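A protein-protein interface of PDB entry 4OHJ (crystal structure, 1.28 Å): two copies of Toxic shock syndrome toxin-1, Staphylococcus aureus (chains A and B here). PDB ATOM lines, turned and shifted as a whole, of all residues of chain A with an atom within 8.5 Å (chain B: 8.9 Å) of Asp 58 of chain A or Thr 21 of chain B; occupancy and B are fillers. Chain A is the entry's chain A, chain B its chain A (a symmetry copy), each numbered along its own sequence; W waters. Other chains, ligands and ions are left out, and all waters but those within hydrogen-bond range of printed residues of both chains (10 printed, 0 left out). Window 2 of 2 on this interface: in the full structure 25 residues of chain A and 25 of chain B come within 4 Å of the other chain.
The backbone carbonyl oxygen (O) of Thr 38 of chain A sits at hydrogen-bond distance from the guanidinium group (NE) of Arg 164 of chain B, at 3.2 Å.
The backbone NH of Thr 21 of chain B sits at hydrogen-bond distance from the backbone carbonyl oxygen of Asp 58 of chain A, 2.9 Å away.
The backbone NH of Asp 58 of chain A lies close to the backbone carbonyl oxygen of Arg 164 of chain B, 3.4 Å away.
The guanidinium group (NH1) of Arg 164 of chain B lies within hydrogen-bond range of the side-chain hydroxyl (OG1) of Thr 40 of chain A, at 3.1 Å.
OD2 of Asp 30 of chain B is in hydrogen-bond range of OH of Tyr 99 of chain A, at 2.5 Å.
The side-chain carboxylate of Asp 30 of chain B is in salt-bridge range of the guanidinium group of Arg 87 of chain A (3.0 Å).
The backbone carbonyl oxygen of Asp 58 of chain A is in hydrogen-bond range of the side-chain amino group of Lys 26 of chain B, at 2.9 Å.
A ring nitrogen (NE2) of His 101 of chain A is in hydrogen-bond range of the side-chain hydroxyl (OG) of Ser 60 of chain A, at 3.3 Å.
The side-chain hydroxyl (OG) of Ser 60 of chain A lies within hydrogen-bond range of the side-chain amide nitrogen (ND2) of Asn 56 of chain A (3.0 Å).
Among the printed residues, pairs that only touch across the chains: Thr 57 of chain A with Arg 164 of chain B (3.6 Å), His 93 of chain A with Asp 23 of chain B (3.6 Å), Tyr 99 of chain A with Lys 26 of chain B (3.9 Å), Asp 58 of chain A with Leu 29 of chain B (3.9 Å), Phe 39 of chain A with Arg 164 of chain B (3.9 Å) and Ser 60 of chain A with Lys 26 of chain B (3.98 Å).
Of chain B, only Thr 21, Lys 26, Leu 29 and Arg 164 come within 4 Å of Asp 58 of chain A.
Thr 21 of chain B touches just one residue of chain A: Asp 58.
No residue of chain B comes within 4 Å of Gly 59 of chain A.
Of the printed residues of chain A, Asp 30 of chain B touches Arg 87 (3.0 Å) and Tyr 99 (2.5 Å).
Printed residues of chain B within 4 Å of Ser 60 of chain A: Lys 26.
Gly 97 of chain A touches none of the printed residues of chain B.
The nearest residue of chain B that does not touch Asp 58 of chain A is Tyr 163 of chain B (4.4 Å).
Of the 19 printed residues of chain A, 9 touch a printed residue of chain B.
Hydrophobic or aromatic side chains of chain A within 4 Å of the printed part of chain B: His 93 and Tyr 99.
Among the printed residues, Asp or Glu carboxylates within 4 Å of a Lys or Arg side-chain nitrogen of the other chain: Arg 87 of chain A with Asp 30 of chain B (3.0 Å).
No position is printed for both chains.
Water W6 lies within hydrogen-bond range of O of Tyr 163 of chain B (2.7 Å), OG1 of Thr 21 of chain B (2.7 Å) and OD2 of Asp 58 of chain A (2.8 Å).
Water W1 lies within hydrogen-bond range of N of Ser 166 of chain B (2.7 Å) and O of Thr 57 of chain A (3.1 Å).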
ATOM      1  N   THR A  38       0.728 -11.526  19.440  1.00  0.00           N
ATOM      2  CA  THR A  38       1.685 -11.178  20.455  1.00  0.00           C
ATOM      3  C   THR A  38       1.554  -9.711  20.775  1.00  0.00           C
ATOM      4  O   THR A  38       1.710  -8.859  19.883  1.00  0.00           O
ATOM      5  CB  THR A  38       3.109 -11.464  19.987  1.00  0.00           C
ATOM      6  OG1 THR A  38       3.171 -12.830  19.571  1.00  0.00           O
ATOM      7  CG2 THR A  38       4.107 -11.218  21.093  1.00  0.00           C
ATOM      8  N   PHE A  39       1.211  -9.401  22.030  1.00  0.00           N
ATOM      9  CA  PHE A  39       1.159  -8.006  22.484  1.00  0.00           C
ATOM     10  C   PHE A  39       1.921  -7.940  23.793  1.00  0.00           C
ATOM     11  O   PHE A  39       1.900  -8.901  24.583  1.00  0.00           O
ATOM     12  CB  PHE A  39      -0.281  -7.484  22.677  1.00  0.00           C
ATOM     13  CG  PHE A  39      -1.059  -7.349  21.411  1.00  0.00           C
ATOM     14  CD1 PHE A  39      -0.907  -6.225  20.629  1.00  0.00           C
ATOM     15  CD2 PHE A  39      -1.967  -8.319  21.023  1.00  0.00           C
ATOM     16  CE1 PHE A  39      -1.625  -6.084  19.437  1.00  0.00           C
ATOM     17  CE2 PHE A  39      -2.679  -8.183  19.830  1.00  0.00           C
ATOM     18  CZ  PHE A  39      -2.528  -7.055  19.074  1.00  0.00           C
ATOM     19  N   THR A  40       2.574  -6.815  24.056  1.00  0.00           N
ATOM     20  CA  THR A  40       3.330  -6.652  25.276  1.00  0.00           C
ATOM     21  C   THR A  40       2.865  -5.433  26.049  1.00  0.00           C
ATOM     22  O   THR A  40       2.576  -4.377  25.454  1.00  0.00           O
ATOM     23  CB  THR A  40       4.823  -6.569  25.022  1.00  0.00           C
ATOM     24  OG1 THR A  40       5.055  -5.679  23.942  1.00  0.00           O
ATOM     25  CG2 THR A  40       5.392  -7.912  24.695  1.00  0.00           C
ATOM     26  N   ASN A  41       2.822  -5.565  27.373  1.00  0.00           N
ATOM     27  CA  ASN A  41       2.484  -4.474  28.269  1.00  0.00           C
ATOM     28  C   ASN A  41       1.102  -3.907  27.983  1.00  0.00           C
ATOM     29  O   ASN A  41       0.893  -2.703  28.066  1.00  0.00           O
ATOM     30  CB  ASN A  41       3.535  -3.392  28.267  1.00  0.00           C
ATOM     31  CG  ASN A  41       3.705  -2.793  29.656  1.00  0.00           C
ATOM     32  OD1 ASN A  41       3.734  -3.520  30.671  1.00  0.00           O
ATOM     33  ND2 ASN A  41       3.852  -1.513  29.718  1.00  0.00           N
ATOM     34  N   SER A  42       0.143  -4.787  27.689  1.00  0.00           N
ATOM     35  CA  SER A  42      -1.242  -4.392  27.548  1.00  0.00           C
ATOM     36  C   SER A  42      -1.794  -4.086  28.950  1.00  0.00           C
ATOM     37  O   SER A  42      -1.232  -4.483  29.965  1.00  0.00           O
ATOM     38  CB  SER A  42      -2.029  -5.515  26.938  1.00  0.00           C
ATOM     39  OG  SER A  42      -1.540  -5.841  25.655  1.00  0.00           O
ATOM     40  N   ILE A  54      -8.953  -6.316  27.716  1.00  0.00           N
ATOM     41  CA  ILE A  54      -7.615  -5.803  27.767  1.00  0.00           C
ATOM     42  C   ILE A  54      -7.358  -4.810  26.657  1.00  0.00           C
ATOM     43  O   ILE A  54      -7.760  -5.026  25.524  1.00  0.00           O
ATOM     44  CB  ILE A  54      -6.639  -7.017  27.640  1.00  0.00           C
ATOM     45  CG1 ILE A  54      -6.724  -7.932  28.876  1.00  0.00           C
ATOM     46  CG2 ILE A  54      -5.232  -6.577  27.439  1.00  0.00           C
ATOM     47  CD1 ILE A  54      -6.199  -9.342  28.631  1.00  0.00           C
ATOM     48  N   LYS A  55      -6.676  -3.712  26.969  1.00  0.00           N
ATOM     49  CA  LYS A  55      -6.314  -2.678  25.982  1.00  0.00           C
ATOM     50  C   LYS A  55      -4.854  -2.817  25.585  1.00  0.00           C
ATOM     51  O   LYS A  55      -3.963  -2.682  26.424  1.00  0.00           O
ATOM     52  CB  LYS A  55      -6.559  -1.265  26.533  1.00  0.00           C
ATOM     53  CG  LYS A  55      -6.210  -0.178  25.518  1.00  0.00           C
ATOM     54  CD  LYS A  55      -6.477   1.221  25.997  1.00  0.00           C
ATOM     55  CE  LYS A  55      -7.963   1.485  26.017  1.00  0.00           C
ATOM     56  NZ  LYS A  55      -8.245   2.901  26.383  1.00  0.00           N
ATOM     57  N   ASN A  56      -4.612  -3.131  24.327  1.00  0.00           N
ATOM     58  CA  ASN A  56      -3.269  -3.281  23.804  1.00  0.00           C
ATOM     59  C   ASN A  56      -2.685  -1.922  23.498  1.00  0.00           C
ATOM     60  O   ASN A  56      -3.420  -0.968  23.250  1.00  0.00           O
ATOM     61  CB  ASN A  56      -3.299  -4.200  22.603  1.00  0.00           C
ATOM     62  CG  ASN A  56      -3.915  -5.538  22.969  1.00  0.00           C
ATOM     63  OD1 ASN A  56      -3.546  -6.160  23.973  1.00  0.00           O
ATOM     64  ND2 ASN A  56      -4.879  -5.992  22.178  1.00  0.00           N
ATOM     65  N   THR A  57      -1.372  -1.819  23.441  1.00  0.00           N
ATOM     66  CA  THR A  57      -0.792  -0.504  23.258  1.00  0.00           C
ATOM     67  C   THR A  57      -0.993   0.036  21.817  1.00  0.00           C
ATOM     68  O   THR A  57      -0.722   1.198  21.571  1.00  0.00           O
ATOM     69  CB  THR A  57       0.664  -0.467  23.693  1.00  0.00           C
ATOM     70  OG1 THR A  57       1.311  -1.435  22.916  1.00  0.00           O
ATOM     71  CG2 THR A  57       0.871  -0.791  25.185  1.00  0.00           C
ATOM     72  N   ASP A  58      -1.429  -0.804  20.868  1.00  0.00           N
ATOM     73  CA  ASP A  58      -1.764  -0.301  19.527  1.00  0.00           C
ATOM     74  C   ASP A  58      -3.186   0.308  19.498  1.00  0.00           C
ATOM     75  O   ASP A  58      -3.632   0.821  18.461  1.00  0.00           O
ATOM     76  CB  ASP A  58      -1.629  -1.315  18.403  1.00  0.00           C
ATOM     77  CG  ASP A  58      -2.664  -2.420  18.437  1.00  0.00           C
ATOM     78  OD1 ASP A  58      -3.361  -2.593  19.463  1.00  0.00           O
ATOM     79  OD2 ASP A  58      -2.801  -3.099  17.403  1.00  0.00           O
ATOM     80  N   GLY A  59      -3.908   0.252  20.625  1.00  0.00           N
ATOM     81  CA  GLY A  59      -5.264   0.784  20.694  1.00  0.00           C
ATOM     82  C   GLY A  59      -6.357  -0.254  20.531  1.00  0.00           C
ATOM     83  O   GLY A  59      -7.537   0.059  20.745  1.00  0.00           O
ATOM     84  N   SER A  60      -6.015  -1.457  20.102  1.00  0.00           N
ATOM     85  CA  SER A  60      -6.988  -2.515  20.016  1.00  0.00           C
ATOM     86  C   SER A  60      -7.371  -3.031  21.389  1.00  0.00           C
ATOM     87  O   SER A  60      -6.653  -2.838  22.369  1.00  0.00           O
ATOM     88  CB  SER A  60      -6.519  -3.677  19.133  1.00  0.00           C
ATOM     89  OG  SER A  60      -5.408  -4.358  19.708  1.00  0.00           O
ATOM     90  N   ILE A  61      -8.509  -3.675  21.439  1.00  0.00           N
ATOM     91  CA  ILE A  61      -9.020  -4.303  22.657  1.00  0.00           C
ATOM     92  C   ILE A  61      -9.100  -5.794  22.438  1.00  0.00           C
ATOM     93  O   ILE A  61      -9.570  -6.244  21.399  1.00  0.00           O
ATOM     94  CB  ILE A  61     -10.446  -3.789  22.970  1.00  0.00           C
ATOM     95  CG1 ILE A  61     -10.459  -2.284  23.096  1.00  0.00           C
ATOM     96  CG2 ILE A  61     -11.072  -4.542  24.143  1.00  0.00           C
ATOM     97  CD1 ILE A  61      -9.743  -1.779  24.282  1.00  0.00           C
ATOM     98  N   SER A  62      -8.588  -6.555  23.397  1.00  0.00           N
ATOM     99  CA  SER A  62      -8.695  -7.994  23.370  1.00  0.00           C
ATOM    100  C   SER A  62      -9.701  -8.474  24.409  1.00  0.00           C
ATOM    101  O   SER A  62      -9.646  -8.095  25.581  1.00  0.00           O
ATOM    102  CB  SER A  62      -7.338  -8.604  23.679  1.00  0.00           C
ATOM    103  OG  SER A  62      -6.459  -8.499  22.587  1.00  0.00           O
ATOM    104  N   ARG A  87      -6.729 -16.314  18.176  1.00  0.00           N
ATOM    105  CA  ARG A  87      -8.078 -15.822  17.941  1.00  0.00           C
ATOM    106  C   ARG A  87      -9.030 -16.964  17.741  1.00  0.00           C
ATOM    107  O   ARG A  87      -8.707 -17.962  17.103  1.00  0.00           O
ATOM    108  CB  ARG A  87      -8.143 -14.976  16.676  1.00  0.00           C
ATOM    109  CG  ARG A  87      -7.398 -13.660  16.790  1.00  0.00           C
ATOM    110  CD  ARG A  87      -7.412 -12.829  15.507  1.00  0.00           C
ATOM    111  NE  ARG A  87      -6.283 -11.893  15.513  1.00  0.00           N
ATOM    112  CZ  ARG A  87      -6.075 -10.844  14.721  1.00  0.00           C
ATOM    113  NH1 ARG A  87      -6.982 -10.450  13.851  1.00  0.00           N
ATOM    114  NH2 ARG A  87      -4.922 -10.189  14.789  1.00  0.00           N
ATOM    115  N   HIS A  93     -14.430  -4.360  13.994  1.00  0.00           N
ATOM    116  CA  HIS A  93     -14.327  -2.957  14.358  1.00  0.00           C
ATOM    117  C   HIS A  93     -15.688  -2.544  14.895  1.00  0.00           C
ATOM    118  O   HIS A  93     -16.735  -2.983  14.405  1.00  0.00           O
ATOM    119  CB  HIS A  93     -13.987  -2.083  13.173  1.00  0.00           C
ATOM    120  CG  HIS A  93     -12.616  -2.289  12.617  1.00  0.00           C
ATOM    121  ND1 HIS A  93     -11.527  -1.570  13.049  1.00  0.00           N
ATOM    122  CD2 HIS A  93     -12.179  -3.075  11.612  1.00  0.00           C
ATOM    123  CE1 HIS A  93     -10.461  -1.935  12.356  1.00  0.00           C
ATOM    124  NE2 HIS A  93     -10.832  -2.844  11.472  1.00  0.00           N
ATOM    125  N   GLY A  97     -15.101   2.740  16.025  1.00  0.00           N
ATOM    126  CA  GLY A  97     -13.860   2.487  15.305  1.00  0.00           C
ATOM    127  C   GLY A  97     -12.835   1.662  16.063  1.00  0.00           C
ATOM    128  O   GLY A  97     -11.719   1.491  15.579  1.00  0.00           O
ATOM    129  N   TYR A  99     -10.975  -1.554  17.362  1.00  0.00           N
ATOM    130  CA  TYR A  99     -10.768  -2.903  16.839  1.00  0.00           C
ATOM    131  C   TYR A  99     -10.746  -3.884  17.993  1.00  0.00           C
ATOM    132  O   TYR A  99      -9.965  -3.749  18.920  1.00  0.00           O
ATOM    133  CB  TYR A  99      -9.469  -2.972  16.052  1.00  0.00           C
ATOM    134  CG  TYR A  99      -9.344  -4.140  15.086  1.00  0.00           C
ATOM    135  CD1 TYR A  99     -10.418  -4.578  14.347  1.00  0.00           C
ATOM    136  CD2 TYR A  99      -8.115  -4.695  14.796  1.00  0.00           C
ATOM    137  CE1 TYR A  99     -10.288  -5.580  13.408  1.00  0.00           C
ATOM    138  CE2 TYR A  99      -7.966  -5.659  13.831  1.00  0.00           C
ATOM    139  CZ  TYR A  99      -9.065  -6.093  13.131  1.00  0.00           C
ATOM    140  OH  TYR A  99      -8.979  -7.081  12.157  1.00  0.00           O
ATOM    141  N   HIS A 101     -10.419  -7.864  19.278  1.00  0.00           N
ATOM    142  CA  HIS A 101      -9.945  -9.205  19.062  1.00  0.00           C
ATOM    143  C   HIS A 101     -10.648 -10.139  20.039  1.00  0.00           C
ATOM    144  O   HIS A 101     -10.898  -9.754  21.178  1.00  0.00           O
ATOM    145  CB  HIS A 101      -8.451  -9.313  19.328  1.00  0.00           C
ATOM    146  CG  HIS A 101      -7.620  -8.399  18.484  1.00  0.00           C
ATOM    147  ND1 HIS A 101      -7.563  -8.498  17.107  1.00  0.00           N
ATOM    148  CD2 HIS A 101      -6.840  -7.344  18.818  1.00  0.00           C
ATOM    149  CE1 HIS A 101      -6.746  -7.560  16.642  1.00  0.00           C
ATOM    150  NE2 HIS A 101      -6.271  -6.866  17.669  1.00  0.00           N
ATOM    151  N   THR B  21      -2.337   2.819  16.828  1.00  0.00           N
ATOM    152  CA  THR B  21      -1.973   2.821  15.387  1.00  0.00           C
ATOM    153  C   THR B  21      -3.227   3.109  14.547  1.00  0.00           C
ATOM    154  O   THR B  21      -4.348   2.991  15.040  1.00  0.00           O
ATOM    155  CB  THR B  21      -1.441   1.443  15.003  1.00  0.00           C
ATOM    156  OG1 THR B  21      -2.416   0.483  15.380  1.00  0.00           O
ATOM    157  CG2 THR B  21      -0.132   1.144  15.727  1.00  0.00           C
ATOM    158  N   ASN B  22      -3.050   3.425  13.266  1.00  0.00           N
ATOM    159  CA  ASN B  22      -4.204   3.656  12.407  1.00  0.00           C
ATOM    160  C   ASN B  22      -4.650   2.320  11.809  1.00  0.00           C
ATOM    161  O   ASN B  22      -3.984   1.275  11.983  1.00  0.00           O
ATOM    162  CB  ASN B  22      -3.907   4.709  11.359  1.00  0.00           C
ATOM    163  CG  ASN B  22      -2.795   4.330  10.452  1.00  0.00           C
ATOM    164  OD1 ASN B  22      -2.567   3.149  10.207  1.00  0.00           O
ATOM    165  ND2 ASN B  22      -2.125   5.328   9.883  1.00  0.00           N
ATOM    166  N   ASP B  23      -5.811   2.326  11.178  1.00  0.00           N
ATOM    167  CA  ASP B  23      -6.372   1.111  10.647  1.00  0.00           C
ATOM    168  C   ASP B  23      -5.535   0.436   9.595  1.00  0.00           C
ATOM    169  O   ASP B  23      -5.532  -0.790   9.540  1.00  0.00           O
ATOM    170  CB  ASP B  23      -7.805   1.324  10.150  1.00  0.00           C
ATOM    171  CG  ASP B  23      -8.801   1.489  11.282  1.00  0.00           C
ATOM    172  OD1 ASP B  23      -8.479   1.120  12.439  1.00  0.00           O
ATOM    173  OD2 ASP B  23      -9.919   1.976  11.003  1.00  0.00           O
ATOM    174  N   ASN B  24      -4.826   1.173   8.766  1.00  0.00           N
ATOM    175  CA  ASN B  24      -4.012   0.470   7.761  1.00  0.00           C
ATOM    176  C   ASN B  24      -2.853  -0.317   8.430  1.00  0.00           C
ATOM    177  O   ASN B  24      -2.460  -1.345   7.944  1.00  0.00           O
ATOM    178  CB  ASN B  24      -3.483   1.392   6.656  1.00  0.00           C
ATOM    179  CG  ASN B  24      -2.164   2.013   6.994  1.00  0.00           C
ATOM    180  OD1 ASN B  24      -1.179   1.828   6.278  1.00  0.00           O
ATOM    181  ND2 ASN B  24      -2.116   2.736   8.088  1.00  0.00           N
ATOM    182  N   ILE B  25      -2.322   0.198   9.525  1.00  0.00           N
ATOM    183  CA  ILE B  25      -1.270  -0.477  10.271  1.00  0.00           C
ATOM    184  C   ILE B  25      -1.878  -1.700  10.977  1.00  0.00           C
ATOM    185  O   ILE B  25      -1.273  -2.756  10.997  1.00  0.00           O
ATOM    186  CB  ILE B  25      -0.588   0.461  11.272  1.00  0.00           C
ATOM    187  CG1 ILE B  25       0.178   1.574  10.535  1.00  0.00           C
ATOM    188  CG2 ILE B  25       0.315  -0.311  12.198  1.00  0.00           C
ATOM    189  CD1 ILE B  25       1.154   1.083   9.494  1.00  0.00           C
ATOM    190  N   LYS B  26      -3.095  -1.586  11.502  1.00  0.00           N
ATOM    191  CA  LYS B  26      -3.738  -2.761  12.097  1.00  0.00           C
ATOM    192  C   LYS B  26      -3.959  -3.825  11.014  1.00  0.00           C
ATOM    193  O   LYS B  26      -3.866  -5.007  11.294  1.00  0.00           O
ATOM    194  CB  LYS B  26      -5.051  -2.395  12.804  1.00  0.00           C
ATOM    195  CG  LYS B  26      -4.834  -1.574  14.058  1.00  0.00           C
ATOM    196  CD  LYS B  26      -6.142  -1.358  14.806  1.00  0.00           C
ATOM    197  CE  LYS B  26      -5.916  -0.743  16.183  1.00  0.00           C
ATOM    198  NZ  LYS B  26      -5.274   0.588  16.093  1.00  0.00           N
ATOM    199  N   ASP B  27      -4.269  -3.395   9.782  1.00  0.00           N
ATOM    200  CA  ASP B  27      -4.451  -4.351   8.673  1.00  0.00           C
ATOM    201  C   ASP B  27      -3.129  -5.052   8.376  1.00  0.00           C
ATOM    202  O   ASP B  27      -3.109  -6.265   8.107  1.00  0.00           O
ATOM    203  CB  ASP B  27      -5.003  -3.691   7.388  1.00  0.00           C
ATOM    204  CG  ASP B  27      -6.478  -3.262   7.489  1.00  0.00           C
ATOM    205  OD1 ASP B  27      -7.251  -3.799   8.313  1.00  0.00           O
ATOM    206  OD2 ASP B  27      -6.887  -2.385   6.685  1.00  0.00           O
ATOM    207  N   LEU B  28      -2.044  -4.296   8.389  1.00  0.00           N
ATOM    208  CA  LEU B  28      -0.713  -4.913   8.177  1.00  0.00           C
ATOM    209  C   LEU B  28      -0.376  -5.912   9.295  1.00  0.00           C
ATOM    210  O   LEU B  28       0.114  -7.017   9.036  1.00  0.00           O
ATOM    211  CB  LEU B  28       0.385  -3.859   8.044  1.00  0.00           C
ATOM    212  CG  LEU B  28       0.365  -3.056   6.733  1.00  0.00           C
ATOM    213  CD1 LEU B  28       1.300  -1.871   6.793  1.00  0.00           C
ATOM    214  CD2 LEU B  28       0.790  -3.911   5.555  1.00  0.00           C
ATOM    215  N   LEU B  29      -0.638  -5.531  10.536  1.00  0.00           N
ATOM    216  CA  LEU B  29      -0.399  -6.436  11.669  1.00  0.00           C
ATOM    217  C   LEU B  29      -1.230  -7.705  11.483  1.00  0.00           C
ATOM    218  O   LEU B  29      -0.720  -8.807  11.659  1.00  0.00           O
ATOM    219  CB  LEU B  29      -0.688  -5.730  12.986  1.00  0.00           C
ATOM    220  CG  LEU B  29      -0.459  -6.611  14.223  1.00  0.00           C
ATOM    221  CD1 LEU B  29       0.961  -7.129  14.303  1.00  0.00           C
ATOM    222  CD2 LEU B  29      -0.834  -5.827  15.456  1.00  0.00           C
ATOM    223  N   ASP B  30      -2.495  -7.582  11.097  1.00  0.00           N
ATOM    224  CA  ASP B  30      -3.311  -8.769  10.876  1.00  0.00           C
ATOM    225  C   ASP B  30      -2.694  -9.677   9.801  1.00  0.00           C
ATOM    226  O   ASP B  30      -2.567 -10.878   9.990  1.00  0.00           O
ATOM    227  CB  ASP B  30      -4.726  -8.408  10.368  1.00  0.00           C
ATOM    228  CG  ASP B  30      -5.670  -7.964  11.419  1.00  0.00           C
ATOM    229  OD1 ASP B  30      -5.407  -8.151  12.627  1.00  0.00           O
ATOM    230  OD2 ASP B  30      -6.781  -7.533  10.997  1.00  0.00           O
ATOM    231  N   GLY B 161       8.307  -5.784  17.540  1.00  0.00           N
ATOM    232  CA  GLY B 161       7.176  -4.886  17.748  1.00  0.00           C
ATOM    233  C   GLY B 161       6.638  -4.129  16.540  1.00  0.00           C
ATOM    234  O   GLY B 161       5.842  -3.231  16.706  1.00  0.00           O
ATOM    235  N   LEU B 162       7.070  -4.495  15.332  1.00  0.00           N
ATOM    236  CA  LEU B 162       6.578  -3.843  14.157  1.00  0.00           C
ATOM    237  C   LEU B 162       5.048  -3.903  14.127  1.00  0.00           C
ATOM    238  O   LEU B 162       4.457  -4.961  14.334  1.00  0.00           O
ATOM    239  CB  LEU B 162       7.173  -4.469  12.883  1.00  0.00           C
ATOM    240  CG  LEU B 162       6.744  -3.849  11.571  1.00  0.00           C
ATOM    241  CD1 LEU B 162       7.255  -2.436  11.416  1.00  0.00           C
ATOM    242  CD2 LEU B 162       7.190  -4.715  10.405  1.00  0.00           C
ATOM    243  N   TYR B 163       4.438  -2.758  13.840  1.00  0.00           N
ATOM    244  CA  TYR B 163       2.972  -2.552  13.714  1.00  0.00           C
ATOM    245  C   TYR B 163       2.212  -2.614  15.045  1.00  0.00           C
ATOM    246  O   TYR B 163       0.994  -2.479  15.063  1.00  0.00           O
ATOM    247  CB  TYR B 163       2.320  -3.516  12.715  1.00  0.00           C
ATOM    248  CG  TYR B 163       2.991  -3.578  11.368  1.00  0.00           C
ATOM    249  CD1 TYR B 163       3.417  -2.435  10.700  1.00  0.00           C
ATOM    250  CD2 TYR B 163       3.176  -4.808  10.737  1.00  0.00           C
ATOM    251  CE1 TYR B 163       4.022  -2.525   9.460  1.00  0.00           C
ATOM    252  CE2 TYR B 163       3.779  -4.896   9.496  1.00  0.00           C
ATOM    253  CZ  TYR B 163       4.181  -3.753   8.852  1.00  0.00           C
ATOM    254  OH  TYR B 163       4.829  -3.866   7.647  1.00  0.00           O
ATOM    255  N   ARG B 164       2.914  -2.785  16.162  1.00  0.00           N
ATOM    256  CA  ARG B 164       2.255  -2.930  17.454  1.00  0.00           C
ATOM    257  C   ARG B 164       2.165  -1.639  18.252  1.00  0.00           C
ATOM    258  O   ARG B 164       1.541  -1.610  19.312  1.00  0.00           O
ATOM    259  CB  ARG B 164       2.900  -4.074  18.262  1.00  0.00           C
ATOM    260  CG  ARG B 164       2.589  -5.414  17.663  1.00  0.00           C
ATOM    261  CD  ARG B 164       3.497  -6.538  18.141  1.00  0.00           C
ATOM    262  NE  ARG B 164       3.838  -6.499  19.547  1.00  0.00           N
ATOM    263  CZ  ARG B 164       4.740  -7.312  20.091  1.00  0.00           C
ATOM    264  NH1 ARG B 164       4.913  -7.332  21.373  1.00  0.00           N
ATOM    265  NH2 ARG B 164       5.407  -8.193  19.363  1.00  0.00           N
ATOM    266  N   SER B 165       2.731  -0.555  17.719  1.00  0.00           N
ATOM    267  CA  SER B 165       2.656   0.727  18.383  1.00  0.00           C
ATOM    268  C   SER B 165       2.946   1.788  17.309  1.00  0.00           C
ATOM    269  O   SER B 165       3.553   1.507  16.278  1.00  0.00           O
ATOM    270  CB  SER B 165       3.592   0.777  19.603  1.00  0.00           C
ATOM    271  OG  SER B 165       4.946   0.568  19.266  1.00  0.00           O
ATOM    272  N   SER B 166       2.520   3.021  17.579  1.00  0.00           N
ATOM    273  CA  SER B 166       2.659   4.134  16.640  1.00  0.00           C
ATOM    274  C   SER B 166       4.108   4.507  16.305  1.00  0.00           C
ATOM    275  O   SER B 166       4.354   5.190  15.308  1.00  0.00           O
ATOM    276  CB  SER B 166       1.946   5.379  17.167  1.00  0.00           C
ATOM    277  OG  SER B 166       2.652   5.908  18.278  1.00  0.00           O
ATOM    278  N   ASP B 167       5.058   4.110  17.142  1.00  0.00           N
ATOM    279  CA  ASP B 167       6.477   4.373  16.876  1.00  0.00           C
ATOM    280  C   ASP B 167       7.168   3.333  15.981  1.00  0.00           C
ATOM    281  O   ASP B 167       8.355   3.479  15.629  1.00  0.00           O
ATOM    282  CB  ASP B 167       7.263   4.475  18.200  1.00  0.00           C
ATOM    283  CG  ASP B 167       7.198   3.194  19.033  1.00  0.00           C
ATOM    284  OD1 ASP B 167       6.086   2.732  19.311  1.00  0.00           O
ATOM    285  OD2 ASP B 167       8.258   2.674  19.439  1.00  0.00           O
ATOM    286  N   LYS B 168       6.433   2.278  15.624  1.00  0.00           N
ATOM    287  CA  LYS B 168       6.977   1.197  14.795  1.00  0.00           C
ATOM    288  C   LYS B 168       5.997   0.896  13.678  1.00  0.00           C
ATOM    289  O   LYS B 168       5.356  -0.145  13.653  1.00  0.00           O
ATOM    290  CB  LYS B 168       7.317  -0.005  15.665  1.00  0.00           C
ATOM    291  CG  LYS B 168       8.419   0.250  16.692  1.00  0.00           C
ATOM    292  CD  LYS B 168       8.749  -1.034  17.427  1.00  0.00           C
ATOM    293  CE  LYS B 168       9.869  -0.787  18.416  1.00  0.00           C
ATOM    294  NZ  LYS B 168      10.260  -1.956  19.243  1.00  0.00           N
ATOM    295  N   THR B 169       5.960   1.790  12.692  1.00  0.00           N
ATOM    296  CA  THR B 169       4.998   1.722  11.613  1.00  0.00           C
ATOM    297  C   THR B 169       5.605   1.781  10.221  1.00  0.00           C
ATOM    298  O   THR B 169       4.890   1.764   9.250  1.00  0.00           O
ATOM    299  CB  THR B 169       4.015   2.886  11.746  1.00  0.00           C
ATOM    300  OG1 THR B 169       4.733   4.122  11.711  1.00  0.00           O
ATOM    301  CG2 THR B 169       3.228   2.799  13.033  1.00  0.00           C
HETATM  302  O   HOH W   1       0.458   3.001  19.341  1.00  0.00           O
HETATM  303  O   HOH W   2      -3.316   3.879  18.954  1.00  0.00           O
HETATM  304  O   HOH W   3       2.677  -4.974  21.795  1.00  0.00           O
HETATM  305  O   HOH W   4       0.549  -3.270  21.149  1.00  0.00           O
HETATM  306  O   HOH W   5      -4.101 -12.021  11.989  1.00  0.00           O
HETATM  307  O   HOH W   6      -1.677  -2.109  15.050  1.00  0.00           O
HETATM  308  O   HOH W   7      -9.990  -5.207   9.772  1.00  0.00           O
HETATM  309  O   HOH W   8      -6.011   3.036  17.865  1.00  0.00           O
HETATM  310  O   HOH W   9      -7.977  -2.143  10.593  1.00  0.00           O
HETATM  311  O   HOH W  10      -3.690  -8.004  15.101  1.00  0.00           O
